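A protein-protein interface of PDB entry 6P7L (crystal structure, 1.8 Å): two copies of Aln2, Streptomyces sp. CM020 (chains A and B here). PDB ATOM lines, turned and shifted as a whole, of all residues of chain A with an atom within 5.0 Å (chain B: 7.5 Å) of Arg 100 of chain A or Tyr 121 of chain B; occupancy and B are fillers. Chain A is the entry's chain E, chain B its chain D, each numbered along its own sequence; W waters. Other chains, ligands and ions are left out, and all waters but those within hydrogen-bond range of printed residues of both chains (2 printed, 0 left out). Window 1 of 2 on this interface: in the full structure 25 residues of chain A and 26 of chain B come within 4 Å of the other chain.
OD2 of Asp 162 of chain B is in salt-bridge range of NE of Arg 100 of chain A (2.9 Å). The backbone carbonyl oxygen (O) of Met 105 of chain B lies within hydrogen-bond range of a ring nitrogen (NE2) of His 49 of chain A (2.8 Å). The side-chain amide oxygen (OE1) of Gln 98 of chain A sits at hydrogen-bond distance from the guanidinium group (NH1) of Arg 169 of chain B. The side-chain hydroxyl (OH) of Tyr 121 of chain B lies within hydrogen-bond range of the backbone carbonyl oxygen (O) of Met 48 of chain A (3.3 Å). NH1 of Arg 100 of chain A sits close to OH of Tyr 121 of chain B. The side-chain hydroxyl (OH) of Tyr 121 of chain B lies within hydrogen-bond range of the side-chain carboxylate (OD2) of Asp 52 of chain A (2.8 Å).
The backbone carbonyl oxygen (O) of Ala 122 of chain B sits at hydrogen-bond distance from the backbone NH (N) of Cys 139 of chain B. The side-chain hydroxyl (OG1) of Thr 138 of chain B is in hydrogen-bond range of the side-chain carboxylate (OD2) of Asp 162 of chain B (2.6 Å). The backbone NH of Tyr 121 of chain B lies within hydrogen-bond range of the backbone carbonyl oxygen of Asp 104 of chain B. The backbone carbonyl oxygen (O) of Thr 125 of chain A sits at hydrogen-bond distance from the backbone NH (N) of Arg 100 of chain A (2.9 Å). OD1 of Asp 52 of chain A is in hydrogen-bond range of ND1 of His 101 of chain A (2.7 Å). The backbone NH (N) of Phe 140 of chain B sits at hydrogen-bond distance from the backbone carbonyl oxygen (O) of Glu 160 of chain B (2.8 Å).
Met 48 of chain A touches Met 105 of chain B. CE1 of His 49 of chain A touches CG2 of Thr 107 of chain B, 3.7 Å away. His 49 of chain A touches Ser 119 of chain B. CG of Gln 98 of chain A touches CG of Asp 162 of chain B, 3.5 Å away. Arg 100 of chain A touches Thr 138 of chain B. Arg 100 of chain A touches Phe 140 of chain B (NH2 to CB, 3.96 Å). O of His 101 of chain A touches CE2 of Tyr 121 of chain B, 3.4 Å away. Trp 102 of chain B touches Trp 102 of chain A. CE3 of Trp 102 of chain A touches CB of Asp 104 of chain B, 3.4 Å away. Thr 123 of chain B touches Trp 102 of chain A.
Pro 99 of chain A touches none of the printed residues of chain B. Arg 100 of chain A touches just these residues of chain B: Tyr 121, Thr 138, Phe 140 and Asp 162. Phe 103 of chain B touches none of the printed residues of chain A. Of the printed residues of chain A, Tyr 121 of chain B touches Met 48, His 49, Asp 52, Arg 100 and His 101. Of the printed residues of chain A, Thr 123 of chain B touches Trp 102. Of the printed residues of chain A, Asp 162 of chain B touches Gln 98 and Arg 100. The nearest residue of chain B that does not touch Arg 100 of chain A is Cys 139 of chain B (5.0 Å).
Of the 12 printed residues of chain A, 8 touch a printed residue of chain B. Among the printed residues, 22 pairs touch across the chains. Among the printed residues, Asp or Glu carboxylates within 4 Å of a Lys or Arg side-chain nitrogen of the other chain: Arg 100 of chain A with Asp 162 of chain B (2.9 Å).
Trp 102 of chain A touches its own counterpart, Trp 102 of chain B. Trp 102 of chain A touches Thr 123 of chain B, but with the chains exchanged Thr 123 of chain A does not touch Trp 102 of chain B (9.9 Å).
Water W1 lies within hydrogen-bond range of the side-chain hydroxyl of Thr 138 of chain B (2.7 Å), the side-chain hydroxyl of Thr 125 of chain A (2.8 Å) and the backbone carbonyl oxygen of Gln 98 of chain A (3.0 Å). Water W2 lies within hydrogen-bond range of OE1 of Gln 98 of chain A (3.1 Å), NH1 of Arg 169 of chain B (3.3 Å) and O of Asp 52 of chain A (3.3 Å).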
ATOM      1  N   MET A  48     -15.045  -2.622  -9.846  1.00  0.00           N
ATOM      2  CA  MET A  48     -16.217  -1.806 -10.131  1.00  0.00           C
ATOM      3  C   MET A  48     -17.062  -1.583  -8.886  1.00  0.00           C
ATOM      4  O   MET A  48     -17.687  -0.528  -8.755  1.00  0.00           O
ATOM      5  CB  MET A  48     -17.061  -2.441 -11.230  1.00  0.00           C
ATOM      6  CG  MET A  48     -16.512  -2.333 -12.613  1.00  0.00           C
ATOM      7  SD  MET A  48     -16.238  -0.614 -13.105  1.00  0.00           S
ATOM      8  CE  MET A  48     -14.540  -0.732 -12.850  1.00  0.00           C
ATOM      9  N   HIS A  49     -17.124  -2.554  -7.964  1.00  0.00           N
ATOM     10  CA  HIS A  49     -17.835  -2.287  -6.712  1.00  0.00           C
ATOM     11  C   HIS A  49     -17.252  -1.063  -6.001  1.00  0.00           C
ATOM     12  O   HIS A  49     -17.987  -0.256  -5.416  1.00  0.00           O
ATOM     13  CB  HIS A  49     -17.767  -3.474  -5.747  1.00  0.00           C
ATOM     14  CG  HIS A  49     -18.586  -4.658  -6.157  1.00  0.00           C
ATOM     15  ND1 HIS A  49     -18.808  -5.732  -5.316  1.00  0.00           N
ATOM     16  CD2 HIS A  49     -19.211  -4.952  -7.320  1.00  0.00           C
ATOM     17  CE1 HIS A  49     -19.527  -6.641  -5.950  1.00  0.00           C
ATOM     18  NE2 HIS A  49     -19.785  -6.194  -7.171  1.00  0.00           N
ATOM     19  N   ASP A  52     -18.185   2.197  -8.097  1.00  0.00           N
ATOM     20  CA  ASP A  52     -19.597   2.514  -7.965  1.00  0.00           C
ATOM     21  C   ASP A  52     -19.981   2.863  -6.534  1.00  0.00           C
ATOM     22  O   ASP A  52     -21.000   3.520  -6.319  1.00  0.00           O
ATOM     23  CB  ASP A  52     -20.436   1.329  -8.440  1.00  0.00           C
ATOM     24  CG  ASP A  52     -20.395   1.149  -9.954  1.00  0.00           C
ATOM     25  OD1 ASP A  52     -20.185   2.139 -10.662  1.00  0.00           O
ATOM     26  OD2 ASP A  52     -20.555   0.019 -10.410  1.00  0.00           O
ATOM     27  N   GLY A  53     -19.224   2.392  -5.557  1.00  0.00           N
ATOM     28  CA  GLY A  53     -19.490   2.657  -4.162  1.00  0.00           C
ATOM     29  C   GLY A  53     -18.786   3.885  -3.633  1.00  0.00           C
ATOM     30  O   GLY A  53     -18.812   4.129  -2.421  1.00  0.00           O
ATOM     31  N   GLN A  98     -27.339   6.671  -8.088  1.00  0.00           N
ATOM     32  CA  GLN A  98     -26.458   5.517  -7.906  1.00  0.00           C
ATOM     33  C   GLN A  98     -26.044   4.888  -9.238  1.00  0.00           C
ATOM     34  O   GLN A  98     -26.898   4.349  -9.972  1.00  0.00           O
ATOM     35  CB  GLN A  98     -27.144   4.478  -7.023  1.00  0.00           C
ATOM     36  CG  GLN A  98     -26.294   3.248  -6.742  1.00  0.00           C
ATOM     37  CD  GLN A  98     -24.979   3.585  -6.057  1.00  0.00           C
ATOM     38  OE1 GLN A  98     -24.961   4.184  -4.985  1.00  0.00           O
ATOM     39  NE2 GLN A  98     -23.864   3.227  -6.692  1.00  0.00           N
ATOM     40  N   PRO A  99     -24.776   4.989  -9.614  1.00  0.00           N
ATOM     41  CA  PRO A  99     -24.309   4.291 -10.815  1.00  0.00           C
ATOM     42  C   PRO A  99     -24.023   2.818 -10.541  1.00  0.00           C
ATOM     43  O   PRO A  99     -23.621   2.421  -9.450  1.00  0.00           O
ATOM     44  CB  PRO A  99     -23.023   5.051 -11.176  1.00  0.00           C
ATOM     45  CG  PRO A  99     -22.455   5.392  -9.759  1.00  0.00           C
ATOM     46  CD  PRO A  99     -23.711   5.793  -8.982  1.00  0.00           C
ATOM     47  N   ARG A 100     -24.199   2.004 -11.584  1.00  0.00           N
ATOM     48  CA  ARG A 100     -23.733   0.625 -11.578  1.00  0.00           C
ATOM     49  C   ARG A 100     -23.121   0.318 -12.938  1.00  0.00           C
ATOM     50  O   ARG A 100     -23.758   0.571 -13.961  1.00  0.00           O
ATOM     51  CB  ARG A 100     -24.867  -0.353 -11.297  1.00  0.00           C
ATOM     52  CG  ARG A 100     -25.461  -0.296  -9.904  1.00  0.00           C
ATOM     53  CD  ARG A 100     -24.509  -0.739  -8.843  1.00  0.00           C
ATOM     54  NE  ARG A 100     -25.066  -0.474  -7.505  1.00  0.00           N
ATOM     55  CZ  ARG A 100     -24.340  -0.385  -6.399  1.00  0.00           C
ATOM     56  NH1 ARG A 100     -23.017  -0.554  -6.445  1.00  0.00           N
ATOM     57  NH2 ARG A 100     -24.932  -0.123  -5.226  1.00  0.00           N
ATOM     58  N   HIS A 101     -21.893  -0.195 -12.945  1.00  0.00           N
ATOM     59  CA  HIS A 101     -21.213  -0.581 -14.175  1.00  0.00           C
ATOM     60  C   HIS A 101     -21.558  -2.021 -14.522  1.00  0.00           C
ATOM     61  O   HIS A 101     -21.596  -2.885 -13.643  1.00  0.00           O
ATOM     62  CB  HIS A 101     -19.707  -0.442 -14.016  1.00  0.00           C
ATOM     63  CG  HIS A 101     -19.211   0.947 -14.198  1.00  0.00           C
ATOM     64  ND1 HIS A 101     -19.374   1.928 -13.246  1.00  0.00           N
ATOM     65  CD2 HIS A 101     -18.544   1.523 -15.226  1.00  0.00           C
ATOM     66  CE1 HIS A 101     -18.814   3.047 -13.672  1.00  0.00           C
ATOM     67  NE2 HIS A 101     -18.316   2.831 -14.878  1.00  0.00           N
ATOM     68  N   TRP A 102     -21.829  -2.264 -15.811  1.00  0.00           N
ATOM     69  CA  TRP A 102     -22.194  -3.571 -16.342  1.00  0.00           C
ATOM     70  C   TRP A 102     -21.173  -3.909 -17.425  1.00  0.00           C
ATOM     71  O   TRP A 102     -21.028  -3.154 -18.398  1.00  0.00           O
ATOM     72  CB  TRP A 102     -23.631  -3.544 -16.913  1.00  0.00           C
ATOM     73  CG  TRP A 102     -24.662  -3.224 -15.875  1.00  0.00           C
ATOM     74  CD1 TRP A 102     -24.982  -1.981 -15.424  1.00  0.00           C
ATOM     75  CD2 TRP A 102     -25.472  -4.146 -15.131  1.00  0.00           C
ATOM     76  NE1 TRP A 102     -25.947  -2.067 -14.443  1.00  0.00           N
ATOM     77  CE2 TRP A 102     -26.268  -3.386 -14.245  1.00  0.00           C
ATOM     78  CE3 TRP A 102     -25.631  -5.538 -15.156  1.00  0.00           C
ATOM     79  CZ2 TRP A 102     -27.188  -3.977 -13.366  1.00  0.00           C
ATOM     80  CZ3 TRP A 102     -26.521  -6.112 -14.291  1.00  0.00           C
ATOM     81  CH2 TRP A 102     -27.316  -5.342 -13.426  1.00  0.00           C
ATOM     82  N   THR A 123     -21.484  -0.580 -19.948  1.00  0.00           N
ATOM     83  CA  THR A 123     -22.377   0.550 -19.801  1.00  0.00           C
ATOM     84  C   THR A 123     -22.512   0.824 -18.314  1.00  0.00           C
ATOM     85  O   THR A 123     -22.019   0.077 -17.478  1.00  0.00           O
ATOM     86  CB  THR A 123     -23.752   0.299 -20.449  1.00  0.00           C
ATOM     87  OG1 THR A 123     -24.531   1.512 -20.400  1.00  0.00           O
ATOM     88  CG2 THR A 123     -24.503  -0.806 -19.753  1.00  0.00           C
ATOM     89  N   VAL A 124     -23.163   1.936 -18.000  1.00  0.00           N
ATOM     90  CA  VAL A 124     -23.469   2.334 -16.641  1.00  0.00           C
ATOM     91  C   VAL A 124     -24.966   2.593 -16.585  1.00  0.00           C
ATOM     92  O   VAL A 124     -25.504   3.281 -17.452  1.00  0.00           O
ATOM     93  CB  VAL A 124     -22.685   3.592 -16.245  1.00  0.00           C
ATOM     94  CG1 VAL A 124     -23.082   4.011 -14.832  1.00  0.00           C
ATOM     95  CG2 VAL A 124     -21.185   3.308 -16.356  1.00  0.00           C
ATOM     96  N   THR A 125     -25.644   1.985 -15.623  1.00  0.00           N
ATOM     97  CA  THR A 125     -27.005   2.391 -15.295  1.00  0.00           C
ATOM     98  C   THR A 125     -26.944   3.404 -14.170  1.00  0.00           C
ATOM     99  O   THR A 125     -26.066   3.348 -13.305  1.00  0.00           O
ATOM    100  CB  THR A 125     -27.870   1.199 -14.878  1.00  0.00           C
ATOM    101  OG1 THR A 125     -27.291   0.528 -13.742  1.00  0.00           O
ATOM    102  CG2 THR A 125     -28.011   0.192 -16.053  1.00  0.00           C
ATOM    103  N   TRP B 102     -31.196  -9.884 -14.515  1.00  0.00           N
ATOM    104  CA  TRP B 102     -29.835  -9.763 -15.026  1.00  0.00           C
ATOM    105  C   TRP B 102     -28.937  -9.594 -13.816  1.00  0.00           C
ATOM    106  O   TRP B 102     -29.176  -8.685 -13.016  1.00  0.00           O
ATOM    107  CB  TRP B 102     -29.702  -8.541 -15.963  1.00  0.00           C
ATOM    108  CG  TRP B 102     -30.633  -8.598 -17.133  1.00  0.00           C
ATOM    109  CD1 TRP B 102     -31.945  -8.270 -17.146  1.00  0.00           C
ATOM    110  CD2 TRP B 102     -30.312  -9.067 -18.448  1.00  0.00           C
ATOM    111  NE1 TRP B 102     -32.486  -8.512 -18.400  1.00  0.00           N
ATOM    112  CE2 TRP B 102     -31.494  -9.001 -19.216  1.00  0.00           C
ATOM    113  CE3 TRP B 102     -29.136  -9.508 -19.061  1.00  0.00           C
ATOM    114  CZ2 TRP B 102     -31.528  -9.355 -20.569  1.00  0.00           C
ATOM    115  CZ3 TRP B 102     -29.178  -9.880 -20.411  1.00  0.00           C
ATOM    116  CH2 TRP B 102     -30.372  -9.809 -21.140  1.00  0.00           C
ATOM    117  N   PHE B 103     -27.938 -10.471 -13.658  1.00  0.00           N
ATOM    118  CA  PHE B 103     -26.901 -10.353 -12.632  1.00  0.00           C
ATOM    119  C   PHE B 103     -25.564 -10.006 -13.283  1.00  0.00           C
ATOM    120  O   PHE B 103     -25.273 -10.417 -14.416  1.00  0.00           O
ATOM    121  CB  PHE B 103     -26.702 -11.652 -11.832  1.00  0.00           C
ATOM    122  CG  PHE B 103     -27.890 -12.113 -11.031  1.00  0.00           C
ATOM    123  CD1 PHE B 103     -29.054 -11.367 -10.928  1.00  0.00           C
ATOM    124  CD2 PHE B 103     -27.816 -13.330 -10.337  1.00  0.00           C
ATOM    125  CE1 PHE B 103     -30.127 -11.826 -10.187  1.00  0.00           C
ATOM    126  CE2 PHE B 103     -28.891 -13.812  -9.580  1.00  0.00           C
ATOM    127  CZ  PHE B 103     -30.050 -13.066  -9.498  1.00  0.00           C
ATOM    128  N   ASP B 104     -24.723  -9.273 -12.560  1.00  0.00           N
ATOM    129  CA  ASP B 104     -23.385  -8.989 -13.078  1.00  0.00           C
ATOM    130  C   ASP B 104     -22.500  -8.546 -11.932  1.00  0.00           C
ATOM    131  O   ASP B 104     -22.972  -8.332 -10.814  1.00  0.00           O
ATOM    132  CB  ASP B 104     -23.462  -7.944 -14.187  1.00  0.00           C
ATOM    133  CG  ASP B 104     -22.253  -7.945 -15.105  1.00  0.00           C
ATOM    134  OD1 ASP B 104     -21.360  -8.799 -14.970  1.00  0.00           O
ATOM    135  OD2 ASP B 104     -22.207  -7.084 -15.986  1.00  0.00           O
ATOM    136  N   MET B 105     -21.191  -8.470 -12.211  1.00  0.00           N
ATOM    137  CA  MET B 105     -20.201  -7.983 -11.234  1.00  0.00           C
ATOM    138  C   MET B 105     -20.256  -8.823  -9.963  1.00  0.00           C
ATOM    139  O   MET B 105     -20.412  -8.300  -8.859  1.00  0.00           O
ATOM    140  CB  MET B 105     -20.422  -6.512 -10.864  1.00  0.00           C
ATOM    141  CG  MET B 105     -20.086  -5.451 -11.881  1.00  0.00           C
ATOM    142  SD  MET B 105     -18.544  -5.663 -12.790  1.00  0.00           S
ATOM    143  CE  MET B 105     -19.497  -6.298 -14.190  1.00  0.00           C
ATOM    144  N   MET B 106     -20.176 -10.137 -10.122  1.00  0.00           N
ATOM    145  CA  MET B 106     -20.427 -11.067  -9.025  1.00  0.00           C
ATOM    146  C   MET B 106     -19.126 -11.517  -8.370  1.00  0.00           C
ATOM    147  O   MET B 106     -18.253 -12.084  -9.031  1.00  0.00           O
ATOM    148  CB  MET B 106     -21.211 -12.283  -9.523  1.00  0.00           C
ATOM    149  CG  MET B 106     -21.348 -13.364  -8.508  1.00  0.00           C
ATOM    150  SD  MET B 106     -22.457 -14.685  -8.917  1.00  0.00           S
ATOM    151  CE  MET B 106     -21.894 -15.366 -10.459  1.00  0.00           C
ATOM    152  N   THR B 107     -19.003 -11.244  -7.067  1.00  0.00           N
ATOM    153  CA  THR B 107     -17.943 -11.787  -6.246  1.00  0.00           C
ATOM    154  C   THR B 107     -18.400 -13.145  -5.722  1.00  0.00           C
ATOM    155  O   THR B 107     -19.579 -13.336  -5.395  1.00  0.00           O
ATOM    156  CB  THR B 107     -17.583 -10.859  -5.088  1.00  0.00           C
ATOM    157  OG1 THR B 107     -18.678 -10.762  -4.170  1.00  0.00           O
ATOM    158  CG2 THR B 107     -17.208  -9.476  -5.613  1.00  0.00           C
ATOM    159  N   SER B 119     -21.739 -11.482  -3.862  1.00  0.00           N
ATOM    160  CA  SER B 119     -22.328 -10.157  -3.923  1.00  0.00           C
ATOM    161  C   SER B 119     -22.383  -9.810  -5.395  1.00  0.00           C
ATOM    162  O   SER B 119     -21.448 -10.119  -6.136  1.00  0.00           O
ATOM    163  CB  SER B 119     -21.543  -9.101  -3.143  1.00  0.00           C
ATOM    164  OG  SER B 119     -20.291  -8.793  -3.712  1.00  0.00           O
ATOM    165  N   TYR B 120     -23.478  -9.197  -5.826  1.00  0.00           N
ATOM    166  CA  TYR B 120     -23.597  -8.884  -7.237  1.00  0.00           C
ATOM    167  C   TYR B 120     -24.585  -7.744  -7.453  1.00  0.00           C
ATOM    168  O   TYR B 120     -25.309  -7.309  -6.547  1.00  0.00           O
ATOM    169  CB  TYR B 120     -24.011 -10.116  -8.056  1.00  0.00           C
ATOM    170  CG  TYR B 120     -25.220 -10.850  -7.516  1.00  0.00           C
ATOM    171  CD1 TYR B 120     -25.083 -11.769  -6.487  1.00  0.00           C
ATOM    172  CD2 TYR B 120     -26.483 -10.647  -8.052  1.00  0.00           C
ATOM    173  CE1 TYR B 120     -26.173 -12.453  -5.984  1.00  0.00           C
ATOM    174  CE2 TYR B 120     -27.588 -11.311  -7.553  1.00  0.00           C
ATOM    175  CZ  TYR B 120     -27.422 -12.236  -6.524  1.00  0.00           C
ATOM    176  OH  TYR B 120     -28.533 -12.905  -6.050  1.00  0.00           O
ATOM    177  N   TYR B 121     -24.539  -7.215  -8.663  1.00  0.00           N
ATOM    178  CA  TYR B 121     -25.525  -6.276  -9.145  1.00  0.00           C
ATOM    179  C   TYR B 121     -26.649  -7.047  -9.814  1.00  0.00           C
ATOM    180  O   TYR B 121     -26.402  -8.015 -10.532  1.00  0.00           O
ATOM    181  CB  TYR B 121     -24.917  -5.332 -10.184  1.00  0.00           C
ATOM    182  CG  TYR B 121     -23.778  -4.477  -9.738  1.00  0.00           C
ATOM    183  CD1 TYR B 121     -23.440  -4.348  -8.395  1.00  0.00           C
ATOM    184  CD2 TYR B 121     -23.031  -3.770 -10.671  1.00  0.00           C
ATOM    185  CE1 TYR B 121     -22.421  -3.528  -7.994  1.00  0.00           C
ATOM    186  CE2 TYR B 121     -21.996  -2.940 -10.283  1.00  0.00           C
ATOM    187  CZ  TYR B 121     -21.699  -2.822  -8.947  1.00  0.00           C
ATOM    188  OH  TYR B 121     -20.661  -2.031  -8.554  1.00  0.00           O
ATOM    189  N   ALA B 122     -27.875  -6.534  -9.671  1.00  0.00           N
ATOM    190  CA  ALA B 122     -29.051  -7.142 -10.278  1.00  0.00           C
ATOM    191  C   ALA B 122     -30.015  -6.065 -10.751  1.00  0.00           C
ATOM    192  O   ALA B 122     -30.143  -5.024 -10.126  1.00  0.00           O
ATOM    193  CB  ALA B 122     -29.760  -8.050  -9.262  1.00  0.00           C
ATOM    194  N   THR B 123     -30.687  -6.320 -11.856  1.00  0.00           N
ATOM    195  CA  THR B 123     -31.833  -5.512 -12.252  1.00  0.00           C
ATOM    196  C   THR B 123     -32.796  -6.473 -12.926  1.00  0.00           C
ATOM    197  O   THR B 123     -32.472  -7.651 -13.160  1.00  0.00           O
ATOM    198  CB  THR B 123     -31.462  -4.365 -13.188  1.00  0.00           C
ATOM    199  OG1 THR B 123     -32.645  -3.599 -13.490  1.00  0.00           O
ATOM    200  CG2 THR B 123     -30.883  -4.921 -14.463  1.00  0.00           C
ATOM    201  N   THR B 138     -31.772  -0.637 -10.026  1.00  0.00           N
ATOM    202  CA  THR B 138     -30.803  -1.666  -9.753  1.00  0.00           C
ATOM    203  C   THR B 138     -30.734  -1.968  -8.260  1.00  0.00           C
ATOM    204  O   THR B 138     -31.154  -1.169  -7.407  1.00  0.00           O
ATOM    205  CB  THR B 138     -29.417  -1.274 -10.275  1.00  0.00           C
ATOM    206  OG1 THR B 138     -29.009  -0.014  -9.739  1.00  0.00           O
ATOM    207  CG2 THR B 138     -29.463  -1.132 -11.759  1.00  0.00           C
ATOM    208  N   CYS B 139     -30.181  -3.145  -7.963  1.00  0.00           N
ATOM    209  CA  CYS B 139     -29.989  -3.651  -6.621  1.00  0.00           C
ATOM    210  C   CYS B 139     -28.545  -4.094  -6.433  1.00  0.00           C
ATOM    211  O   CYS B 139     -27.891  -4.555  -7.378  1.00  0.00           O
ATOM    212  CB  CYS B 139     -30.911  -4.881  -6.341  1.00  0.00           C
ATOM    213  SG  CYS B 139     -32.684  -4.482  -6.379  1.00  0.00           S
ATOM    214  N   PHE B 140     -28.089  -4.015  -5.193  1.00  0.00           N
ATOM    215  CA  PHE B 140     -26.872  -4.677  -4.745  1.00  0.00           C
ATOM    216  C   PHE B 140     -27.316  -5.841  -3.867  1.00  0.00           C
ATOM    217  O   PHE B 140     -28.061  -5.630  -2.898  1.00  0.00           O
ATOM    218  CB  PHE B 140     -25.962  -3.733  -3.970  1.00  0.00           C
ATOM    219  CG  PHE B 140     -24.642  -4.337  -3.626  1.00  0.00           C
ATOM    220  CD1 PHE B 140     -23.641  -4.427  -4.568  1.00  0.00           C
ATOM    221  CD2 PHE B 140     -24.395  -4.813  -2.355  1.00  0.00           C
ATOM    222  CE1 PHE B 140     -22.416  -4.972  -4.237  1.00  0.00           C
ATOM    223  CE2 PHE B 140     -23.186  -5.378  -2.039  1.00  0.00           C
ATOM    224  CZ  PHE B 140     -22.205  -5.471  -2.974  1.00  0.00           C
ATOM    225  N   VAL B 141     -26.941  -7.055  -4.259  1.00  0.00           N
ATOM    226  CA  VAL B 141     -27.445  -8.278  -3.622  1.00  0.00           C
ATOM    227  C   VAL B 141     -26.295  -8.999  -2.938  1.00  0.00           C
ATOM    228  O   VAL B 141     -25.220  -9.153  -3.518  1.00  0.00           O
ATOM    229  CB  VAL B 141     -28.135  -9.200  -4.648  1.00  0.00           C
ATOM    230  CG1 VAL B 141     -28.770 -10.409  -3.953  1.00  0.00           C
ATOM    231  CG2 VAL B 141     -29.180  -8.405  -5.459  1.00  0.00           C
ATOM    232  N   GLU B 160     -30.471  -4.889  -1.432  1.00  0.00           N
ATOM    233  CA  GLU B 160     -30.392  -3.443  -1.213  1.00  0.00           C
ATOM    234  C   GLU B 160     -30.803  -2.778  -2.520  1.00  0.00           C
ATOM    235  O   GLU B 160     -30.104  -2.925  -3.527  1.00  0.00           O
ATOM    236  CB  GLU B 160     -28.980  -3.008  -0.830  1.00  0.00           C
ATOM    237  CG  GLU B 160     -28.500  -3.461   0.535  1.00  0.00           C
ATOM    238  CD  GLU B 160     -28.238  -2.299   1.481  1.00  0.00           C
ATOM    239  OE1 GLU B 160     -27.893  -1.193   1.010  1.00  0.00           O
ATOM    240  OE2 GLU B 160     -28.389  -2.492   2.704  1.00  0.00           O
ATOM    241  N   ARG B 161     -31.927  -2.065  -2.528  1.00  0.00           N
ATOM    242  CA  ARG B 161     -32.411  -1.427  -3.749  1.00  0.00           C
ATOM    243  C   ARG B 161     -31.810  -0.030  -3.854  1.00  0.00           C
ATOM    244  O   ARG B 161     -31.846   0.759  -2.892  1.00  0.00           O
ATOM    245  CB  ARG B 161     -33.944  -1.393  -3.806  1.00  0.00           C
ATOM    246  CG  ARG B 161     -34.424  -1.660  -5.243  1.00  0.00           C
ATOM    247  CD  ARG B 161     -35.905  -1.916  -5.341  1.00  0.00           C
ATOM    248  NE  ARG B 161     -36.658  -0.704  -5.065  1.00  0.00           N
ATOM    249  CZ  ARG B 161     -37.932  -0.682  -4.682  1.00  0.00           C
ATOM    250  NH1 ARG B 161     -38.602  -1.817  -4.532  1.00  0.00           N
ATOM    251  NH2 ARG B 161     -38.531   0.480  -4.457  1.00  0.00           N
ATOM    252  N   ASP B 162     -31.217   0.244  -5.017  1.00  0.00           N
ATOM    253  CA  ASP B 162     -30.400   1.431  -5.176  1.00  0.00           C
ATOM    254  C   ASP B 162     -31.218   2.712  -5.086  1.00  0.00           C
ATOM    255  O   ASP B 162     -30.703   3.724  -4.601  1.00  0.00           O
ATOM    256  CB  ASP B 162     -29.640   1.359  -6.508  1.00  0.00           C
ATOM    257  CG  ASP B 162     -28.363   0.493  -6.409  1.00  0.00           C
ATOM    258  OD1 ASP B 162     -27.827   0.315  -5.301  1.00  0.00           O
ATOM    259  OD2 ASP B 162     -27.887  -0.041  -7.426  1.00  0.00           O
ATOM    260  N   VAL B 165     -31.537   3.394  -1.372  1.00  0.00           N
ATOM    261  CA  VAL B 165     -30.288   3.891  -0.802  1.00  0.00           C
ATOM    262  C   VAL B 165     -30.096   5.365  -1.137  1.00  0.00           C
ATOM    263  O   VAL B 165     -29.752   6.180  -0.263  1.00  0.00           O
ATOM    264  CB  VAL B 165     -29.102   3.052  -1.303  1.00  0.00           C
ATOM    265  CG1 VAL B 165     -27.780   3.693  -0.897  1.00  0.00           C
ATOM    266  CG2 VAL B 165     -29.222   1.629  -0.784  1.00  0.00           C
ATOM    267  N   ARG B 169     -29.956   8.953   1.468  1.00  0.00           N
ATOM    268  CA  ARG B 169     -28.733   9.723   1.650  1.00  0.00           C
ATOM    269  C   ARG B 169     -28.833  11.123   1.072  1.00  0.00           C
ATOM    270  O   ARG B 169     -29.845  11.498   0.475  1.00  0.00           O
ATOM    271  CB  ARG B 169     -27.550   8.984   1.005  1.00  0.00           C
ATOM    272  CG  ARG B 169     -27.491   9.105  -0.522  1.00  0.00           C
ATOM    273  CD  ARG B 169     -26.751   7.930  -1.152  1.00  0.00           C
ATOM    274  NE  ARG B 169     -26.352   8.197  -2.534  1.00  0.00           N
ATOM    275  CZ  ARG B 169     -25.682   7.342  -3.302  1.00  0.00           C
ATOM    276  NH1 ARG B 169     -25.334   6.154  -2.828  1.00  0.00           N
ATOM    277  NH2 ARG B 169     -25.352   7.674  -4.543  1.00  0.00           N
HETATM  278  O   HOH W   1     -28.013   1.923 -11.404  1.00  0.00           O
HETATM  279  O   HOH W   2     -22.381   5.804  -4.297  1.00  0.00           O
